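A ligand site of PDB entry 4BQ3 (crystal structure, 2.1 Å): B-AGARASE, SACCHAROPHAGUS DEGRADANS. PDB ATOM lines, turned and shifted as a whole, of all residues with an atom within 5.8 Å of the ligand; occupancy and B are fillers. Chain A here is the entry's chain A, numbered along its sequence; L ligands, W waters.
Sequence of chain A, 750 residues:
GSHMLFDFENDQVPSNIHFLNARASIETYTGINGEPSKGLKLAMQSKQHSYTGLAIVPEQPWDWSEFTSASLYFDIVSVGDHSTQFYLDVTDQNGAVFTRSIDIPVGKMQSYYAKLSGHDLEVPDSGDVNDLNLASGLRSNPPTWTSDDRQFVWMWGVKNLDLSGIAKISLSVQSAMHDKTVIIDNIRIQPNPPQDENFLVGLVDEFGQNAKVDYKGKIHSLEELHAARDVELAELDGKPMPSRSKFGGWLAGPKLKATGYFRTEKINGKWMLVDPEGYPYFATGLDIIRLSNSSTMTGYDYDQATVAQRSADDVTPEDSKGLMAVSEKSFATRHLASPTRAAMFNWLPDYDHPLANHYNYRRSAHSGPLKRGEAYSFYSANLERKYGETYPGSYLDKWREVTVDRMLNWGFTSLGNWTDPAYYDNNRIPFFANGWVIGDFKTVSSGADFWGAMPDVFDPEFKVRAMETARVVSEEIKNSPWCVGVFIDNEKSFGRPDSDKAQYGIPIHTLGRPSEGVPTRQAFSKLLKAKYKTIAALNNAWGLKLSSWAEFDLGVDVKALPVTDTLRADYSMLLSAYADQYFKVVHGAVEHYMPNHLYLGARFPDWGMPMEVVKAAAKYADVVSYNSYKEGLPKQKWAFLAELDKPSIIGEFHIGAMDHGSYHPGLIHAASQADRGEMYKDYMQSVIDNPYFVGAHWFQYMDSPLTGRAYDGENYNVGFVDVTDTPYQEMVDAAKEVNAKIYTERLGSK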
ATOM      1  N   ARG A 139      14.532  -8.858   6.176  1.00  0.00           N
ATOM      2  CA  ARG A 139      15.408  -8.228   7.150  1.00  0.00           C
ATOM      3  C   ARG A 139      14.691  -8.199   8.501  1.00  0.00           C
ATOM      4  O   ARG A 139      15.301  -8.433   9.525  1.00  0.00           O
ATOM      5  CB  ARG A 139      15.898  -6.832   6.715  1.00  0.00           C
ATOM      6  CG  ARG A 139      16.954  -6.216   7.686  1.00  0.00           C
ATOM      7  CD  ARG A 139      18.247  -7.059   7.788  1.00  0.00           C
ATOM      8  NE  ARG A 139      18.725  -7.446   6.456  1.00  0.00           N
ATOM      9  CZ  ARG A 139      19.538  -6.721   5.682  1.00  0.00           C
ATOM     10  NH1 ARG A 139      20.007  -5.547   6.094  1.00  0.00           N
ATOM     11  NH2 ARG A 139      19.874  -7.177   4.459  1.00  0.00           N
ATOM     12  N   TRP A 156      20.485  -5.598  13.342  1.00  0.00           N
ATOM     13  CA  TRP A 156      21.706  -6.419  13.140  1.00  0.00           C
ATOM     14  C   TRP A 156      22.174  -6.950  14.497  1.00  0.00           C
ATOM     15  O   TRP A 156      21.707  -6.485  15.552  1.00  0.00           O
ATOM     16  CB  TRP A 156      22.857  -5.584  12.499  1.00  0.00           C
ATOM     17  CG  TRP A 156      22.928  -4.129  13.044  1.00  0.00           C
ATOM     18  CD1 TRP A 156      23.472  -3.692  14.244  1.00  0.00           C
ATOM     19  CD2 TRP A 156      22.430  -2.953  12.390  1.00  0.00           C
ATOM     20  NE1 TRP A 156      23.329  -2.319  14.363  1.00  0.00           N
ATOM     21  CE2 TRP A 156      22.705  -1.847  13.238  1.00  0.00           C
ATOM     22  CE3 TRP A 156      21.836  -2.712  11.135  1.00  0.00           C
ATOM     23  CZ2 TRP A 156      22.366  -0.521  12.869  1.00  0.00           C
ATOM     24  CZ3 TRP A 156      21.504  -1.422  10.793  1.00  0.00           C
ATOM     25  CH2 TRP A 156      21.766  -0.342  11.659  1.00  0.00           C
ATOM     26  N   GLY A 157      23.106  -7.912  14.461  1.00  0.00           N
ATOM     27  CA  GLY A 157      23.756  -8.401  15.658  1.00  0.00           C
ATOM     28  C   GLY A 157      23.465  -9.896  15.919  1.00  0.00           C
ATOM     29  O   GLY A 157      23.033 -10.609  15.020  1.00  0.00           O
ATOM     30  N   PHE A 450      32.139  -6.148   4.826  1.00  0.00           N
ATOM     31  CA  PHE A 450      30.674  -6.240   4.796  1.00  0.00           C
ATOM     32  C   PHE A 450      30.112  -6.765   3.473  1.00  0.00           C
ATOM     33  O   PHE A 450      29.595  -7.873   3.447  1.00  0.00           O
ATOM     34  CB  PHE A 450      30.011  -4.954   5.218  1.00  0.00           C
ATOM     35  CG  PHE A 450      28.508  -5.076   5.344  1.00  0.00           C
ATOM     36  CD1 PHE A 450      27.686  -4.887   4.227  1.00  0.00           C
ATOM     37  CD2 PHE A 450      27.913  -5.357   6.589  1.00  0.00           C
ATOM     38  CE1 PHE A 450      26.293  -5.007   4.337  1.00  0.00           C
ATOM     39  CE2 PHE A 450      26.512  -5.456   6.696  1.00  0.00           C
ATOM     40  CZ  PHE A 450      25.714  -5.305   5.563  1.00  0.00           C
ATOM     41  N   TRP A 451      30.241  -6.011   2.392  1.00  0.00           N
ATOM     42  CA  TRP A 451      29.706  -6.450   1.099  1.00  0.00           C
ATOM     43  C   TRP A 451      30.533  -7.510   0.366  1.00  0.00           C
ATOM     44  O   TRP A 451      30.006  -8.218  -0.478  1.00  0.00           O
ATOM     45  CB  TRP A 451      29.540  -5.276   0.138  1.00  0.00           C
ATOM     46  CG  TRP A 451      28.434  -4.337   0.556  1.00  0.00           C
ATOM     47  CD1 TRP A 451      28.564  -3.024   0.926  1.00  0.00           C
ATOM     48  CD2 TRP A 451      27.032  -4.657   0.689  1.00  0.00           C
ATOM     49  NE1 TRP A 451      27.337  -2.500   1.224  1.00  0.00           N
ATOM     50  CE2 TRP A 451      26.381  -3.486   1.113  1.00  0.00           C
ATOM     51  CE3 TRP A 451      26.278  -5.846   0.488  1.00  0.00           C
ATOM     52  CZ2 TRP A 451      24.989  -3.441   1.353  1.00  0.00           C
ATOM     53  CZ3 TRP A 451      24.894  -5.805   0.717  1.00  0.00           C
ATOM     54  CH2 TRP A 451      24.268  -4.606   1.142  1.00  0.00           C
ATOM     55  N   GLU A 491      30.418   1.747  -0.686  1.00  0.00           N
ATOM     56  CA  GLU A 491      30.479   1.171   0.648  1.00  0.00           C
ATOM     57  C   GLU A 491      31.519   0.052   0.795  1.00  0.00           C
ATOM     58  O   GLU A 491      31.232  -1.078   1.288  1.00  0.00           O
ATOM     59  CB  GLU A 491      29.064   0.738   1.087  1.00  0.00           C
ATOM     60  CG  GLU A 491      28.072   1.912   1.200  1.00  0.00           C
ATOM     61  CD  GLU A 491      26.665   1.483   1.615  1.00  0.00           C
ATOM     62  OE1 GLU A 491      26.392   0.256   1.837  1.00  0.00           O
ATOM     63  OE2 GLU A 491      25.809   2.397   1.671  1.00  0.00           O
ATOM     64  N   ARG A 496      36.405  -0.096  10.001  1.00  0.00           N
ATOM     65  CA  ARG A 496      35.356   0.402  10.908  1.00  0.00           C
ATOM     66  C   ARG A 496      35.906   1.356  11.975  1.00  0.00           C
ATOM     67  O   ARG A 496      37.078   1.277  12.345  1.00  0.00           O
ATOM     68  CB  ARG A 496      34.555  -0.767  11.517  1.00  0.00           C
ATOM     69  CG  ARG A 496      33.689  -1.407  10.460  1.00  0.00           C
ATOM     70  CD  ARG A 496      32.514  -2.159  11.045  1.00  0.00           C
ATOM     71  NE  ARG A 496      31.651  -2.632   9.953  1.00  0.00           N
ATOM     72  CZ  ARG A 496      30.325  -2.577   9.963  1.00  0.00           C
ATOM     73  NH1 ARG A 496      29.674  -2.040  10.999  1.00  0.00           N
ATOM     74  NH2 ARG A 496      29.631  -3.033   8.904  1.00  0.00           N
ATOM     75  N   PRO A 605      30.313   4.842   3.657  1.00  0.00           N
ATOM     76  CA  PRO A 605      29.323   4.763   4.742  1.00  0.00           C
ATOM     77  C   PRO A 605      29.937   5.213   6.083  1.00  0.00           C
ATOM     78  O   PRO A 605      31.159   5.331   6.175  1.00  0.00           O
ATOM     79  CB  PRO A 605      29.011   3.276   4.808  1.00  0.00           C
ATOM     80  CG  PRO A 605      30.312   2.624   4.444  1.00  0.00           C
ATOM     81  CD  PRO A 605      30.999   3.544   3.461  1.00  0.00           C
ATOM     82  N   ASP A 606      29.109   5.482   7.110  1.00  0.00           N
ATOM     83  CA  ASP A 606      29.649   5.874   8.424  1.00  0.00           C
ATOM     84  C   ASP A 606      30.570   4.795   8.983  1.00  0.00           C
ATOM     85  O   ASP A 606      31.482   5.110   9.741  1.00  0.00           O
ATOM     86  CB  ASP A 606      28.531   6.172   9.456  1.00  0.00           C
ATOM     87  CG  ASP A 606      27.682   4.933   9.829  1.00  0.00           C
ATOM     88  OD1 ASP A 606      27.282   4.141   8.963  1.00  0.00           O
ATOM     89  OD2 ASP A 606      27.333   4.778  11.000  1.00  0.00           O
ATOM     90  N   TRP A 607      30.364   3.531   8.603  1.00  0.00           N
ATOM     91  CA  TRP A 607      31.221   2.471   9.117  1.00  0.00           C
ATOM     92  C   TRP A 607      32.494   2.191   8.253  1.00  0.00           C
ATOM     93  O   TRP A 607      33.153   1.189   8.463  1.00  0.00           O
ATOM     94  CB  TRP A 607      30.437   1.153   9.279  1.00  0.00           C
ATOM     95  CG  TRP A 607      29.478   0.778   8.107  1.00  0.00           C
ATOM     96  CD1 TRP A 607      28.137   1.122   8.016  1.00  0.00           C
ATOM     97  CD2 TRP A 607      29.794   0.057   6.892  1.00  0.00           C
ATOM     98  NE1 TRP A 607      27.616   0.632   6.825  1.00  0.00           N
ATOM     99  CE2 TRP A 607      28.615  -0.009   6.121  1.00  0.00           C
ATOM    100  CE3 TRP A 607      30.988  -0.515   6.372  1.00  0.00           C
ATOM    101  CZ2 TRP A 607      28.561  -0.665   4.885  1.00  0.00           C
ATOM    102  CZ3 TRP A 607      30.951  -1.132   5.135  1.00  0.00           C
ATOM    103  CH2 TRP A 607      29.733  -1.206   4.392  1.00  0.00           C
ATOM    104  N   TYR A 629      22.988   7.338   6.684  1.00  0.00           N
ATOM    105  CA  TYR A 629      21.691   7.052   7.156  1.00  0.00           C
ATOM    106  C   TYR A 629      21.525   7.527   8.598  1.00  0.00           C
ATOM    107  O   TYR A 629      21.697   6.775   9.551  1.00  0.00           O
ATOM    108  CB  TYR A 629      21.461   5.534   7.000  1.00  0.00           C
ATOM    109  CG  TYR A 629      21.308   5.126   5.529  1.00  0.00           C
ATOM    110  CD1 TYR A 629      20.119   5.423   4.795  1.00  0.00           C
ATOM    111  CD2 TYR A 629      22.368   4.480   4.838  1.00  0.00           C
ATOM    112  CE1 TYR A 629      19.997   5.050   3.446  1.00  0.00           C
ATOM    113  CE2 TYR A 629      22.237   4.104   3.512  1.00  0.00           C
ATOM    114  CZ  TYR A 629      21.061   4.371   2.834  1.00  0.00           C
ATOM    115  OH  TYR A 629      20.968   3.978   1.506  1.00  0.00           O
ATOM    116  N   LYS A 630      21.186   8.806   8.736  1.00  0.00           N
ATOM    117  CA  LYS A 630      21.038   9.447  10.016  1.00  0.00           C
ATOM    118  C   LYS A 630      19.885  10.460   9.836  1.00  0.00           C
ATOM    119  O   LYS A 630      19.343  10.619   8.704  1.00  0.00           O
ATOM    120  CB  LYS A 630      22.326  10.198  10.417  1.00  0.00           C
ATOM    121  CG  LYS A 630      23.648   9.405  10.348  1.00  0.00           C
ATOM    122  CD  LYS A 630      23.805   8.373  11.467  1.00  0.00           C
ATOM    123  CE  LYS A 630      25.082   7.530  11.251  1.00  0.00           C
ATOM    124  NZ  LYS A 630      24.994   6.195  11.912  1.00  0.00           N
ATOM    125  N   GLU A 652      23.434   8.664  -0.428  1.00  0.00           N
ATOM    126  CA  GLU A 652      22.287   7.928   0.108  1.00  0.00           C
ATOM    127  C   GLU A 652      21.879   8.439   1.434  1.00  0.00           C
ATOM    128  O   GLU A 652      22.727   8.670   2.282  1.00  0.00           O
ATOM    129  CB  GLU A 652      22.618   6.427   0.299  1.00  0.00           C
ATOM    130  CG  GLU A 652      23.139   5.742  -0.955  1.00  0.00           C
ATOM    131  CD  GLU A 652      23.451   4.259  -0.786  1.00  0.00           C
ATOM    132  OE1 GLU A 652      23.292   3.665   0.347  1.00  0.00           O
ATOM    133  OE2 GLU A 652      23.895   3.691  -1.805  1.00  0.00           O
ATOM    134  N   LEU A 667      16.462   2.187   7.463  1.00  0.00           N
ATOM    135  CA  LEU A 667      17.503   2.469   8.415  1.00  0.00           C
ATOM    136  C   LEU A 667      17.182   3.550   9.440  1.00  0.00           C
ATOM    137  O   LEU A 667      17.657   3.465  10.586  1.00  0.00           O
ATOM    138  CB  LEU A 667      18.845   2.765   7.706  1.00  0.00           C
ATOM    139  CG  LEU A 667      19.373   1.466   7.018  1.00  0.00           C
ATOM    140  CD1 LEU A 667      20.505   1.766   6.071  1.00  0.00           C
ATOM    141  CD2 LEU A 667      19.778   0.407   8.032  1.00  0.00           C
ATOM    142  N   GLU A 714      16.617  -6.870   2.109  1.00  0.00           N
ATOM    143  CA  GLU A 714      16.117  -5.593   2.632  1.00  0.00           C
ATOM    144  C   GLU A 714      14.659  -5.478   2.205  1.00  0.00           C
ATOM    145  O   GLU A 714      14.327  -5.768   1.046  1.00  0.00           O
ATOM    146  CB  GLU A 714      16.936  -4.381   2.126  1.00  0.00           C
ATOM    147  CG  GLU A 714      18.399  -4.355   2.584  1.00  0.00           C
ATOM    148  CD  GLU A 714      19.122  -3.079   2.119  1.00  0.00           C
ATOM    149  OE1 GLU A 714      18.484  -2.274   1.390  1.00  0.00           O
ATOM    150  OE2 GLU A 714      20.294  -2.852   2.516  1.00  0.00           O
ATOM    151  N   TYR A 716      12.311  -2.575   2.821  1.00  0.00           N
ATOM    152  CA  TYR A 716      12.108  -1.326   3.482  1.00  0.00           C
ATOM    153  C   TYR A 716      11.113  -0.386   2.818  1.00  0.00           C
ATOM    154  O   TYR A 716      11.030  -0.342   1.591  1.00  0.00           O
ATOM    155  CB  TYR A 716      13.433  -0.624   3.474  1.00  0.00           C
ATOM    156  CG  TYR A 716      14.573  -1.294   4.223  1.00  0.00           C
ATOM    157  CD1 TYR A 716      14.356  -2.276   5.211  1.00  0.00           C
ATOM    158  CD2 TYR A 716      15.890  -0.902   3.953  1.00  0.00           C
ATOM    159  CE1 TYR A 716      15.450  -2.857   5.876  1.00  0.00           C
ATOM    160  CE2 TYR A 716      16.960  -1.446   4.624  1.00  0.00           C
ATOM    161  CZ  TYR A 716      16.756  -2.393   5.591  1.00  0.00           C
ATOM    162  OH  TYR A 716      17.859  -2.875   6.285  1.00  0.00           O
HETATM  163  O1  LIG L   1      24.745   1.402   6.664  1.00  0.00           O
HETATM  164  C1  LIG L   1      23.782   0.366   6.648  1.00  0.00           C
HETATM  165  C2  LIG L   1      23.387   0.002   5.224  1.00  0.00           C
HETATM  166  C3  LIG L   1      24.649  -0.440   4.500  1.00  0.00           C
HETATM  167  O2  LIG L   1      24.334  -0.510   3.095  1.00  0.00           O
HETATM  168  O3  LIG L   1      22.606  -1.225   5.377  1.00  0.00           O
HETATM  169  C4  LIG L   1      23.458  -2.435   5.076  1.00  0.00           C
HETATM  170  C5  LIG L   1      24.883  -1.831   5.105  1.00  0.00           C
HETATM  171  O4  LIG L   1      25.276  -1.625   6.470  1.00  0.00           O
HETATM  172  C6  LIG L   1      24.356  -0.872   7.345  1.00  0.00           C
HETATM  173  O5  LIG L   1      25.071  -0.347   8.490  1.00  0.00           O
HETATM  174  C7  LIG L   1      25.086  -1.223   9.575  1.00  0.00           C
HETATM  175  C8  LIG L   1      25.659  -2.613   9.230  1.00  0.00           C
HETATM  176  O6  LIG L   1      26.929  -2.482   8.568  1.00  0.00           O
HETATM  177  C9  LIG L   1      25.904  -3.370  10.556  1.00  0.00           C
HETATM  178  C10 LIG L   1      26.597  -4.675  10.247  1.00  0.00           C
HETATM  179  O7  LIG L   1      26.039  -5.542  11.219  1.00  0.00           O
HETATM  180  O8  LIG L   1      26.759  -2.621  11.455  1.00  0.00           O
HETATM  181  C11 LIG L   1      26.145  -1.429  11.901  1.00  0.00           C
HETATM  182  O9  LIG L   1      27.130  -0.854  12.747  1.00  0.00           O
HETATM  183  C12 LIG L   1      26.006  -0.560  10.629  1.00  0.00           C
HETATM  184  O10 LIG L   1      25.474   0.686  10.999  1.00  0.00           O
HETATM  185  O   HOH W   1      24.957   2.842   8.990  1.00  0.00           O
HETATM  186  O   HOH W   2      21.561  -4.919   3.743  1.00  0.00           O
HETATM  187  O   HOH W   3      27.090   2.572  11.965  1.00  0.00           O
HETATM  188  O   HOH W   4      25.556   3.186   4.578  1.00  0.00           O
HETATM  189  O   HOH W   5      20.243  -2.477   5.275  1.00  0.00           O
HETATM  190  O   HOH W   6      27.710  -2.247  14.779  1.00  0.00           O
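O2 of the ligand sits at hydrogen-bond distance from OE1 of Glu 491, 2.5 Å away. The guanidinium group of Arg 496 is in hydrogen-bond range of an oxygen (O6) of the ligand. NE1 of Trp 607 lies within hydrogen-bond range of O1 of the ligand (3.0 Å).
The side-chain carboxylate of Glu 491 lies within hydrogen-bond range of the indole nitrogen of Trp 451.
CB of Trp 156 touches O7 of the ligand (3.4 Å). Phe 450 touches the ligand (CE2 to O6, 3.5 Å). Trp 451 touches the ligand (CZ2 to O2, 3.5 Å). Leu 667 touches the ligand. Hydrophobic or aromatic side chains within 4 Å of the ligand: Trp 156, Phe 450, Trp 451, Trp 607 and Leu 667.
Water W3 bridges OD2 of Asp 606 (2.4 Å) and O10 of the ligand (2.7 Å). Water W5 lies within hydrogen-bond range of OH of Tyr 716, O3 of the ligand, OE2 of Glu 714 and NH1 of Arg 139. Water W1 lies within hydrogen-bond range of the side-chain carboxylate (OD1) of Asp 606 (2.7 Å) and an oxygen (O1) of the ligand (2.7 Å). Water W4 bridges O1 of the ligand (2.9 Å) and OE2 of Glu 491 (3.0 Å). Water W2 bridges OE2 of Glu 714 (2.7 Å) and NH1 of Arg 139 (2.9 Å).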
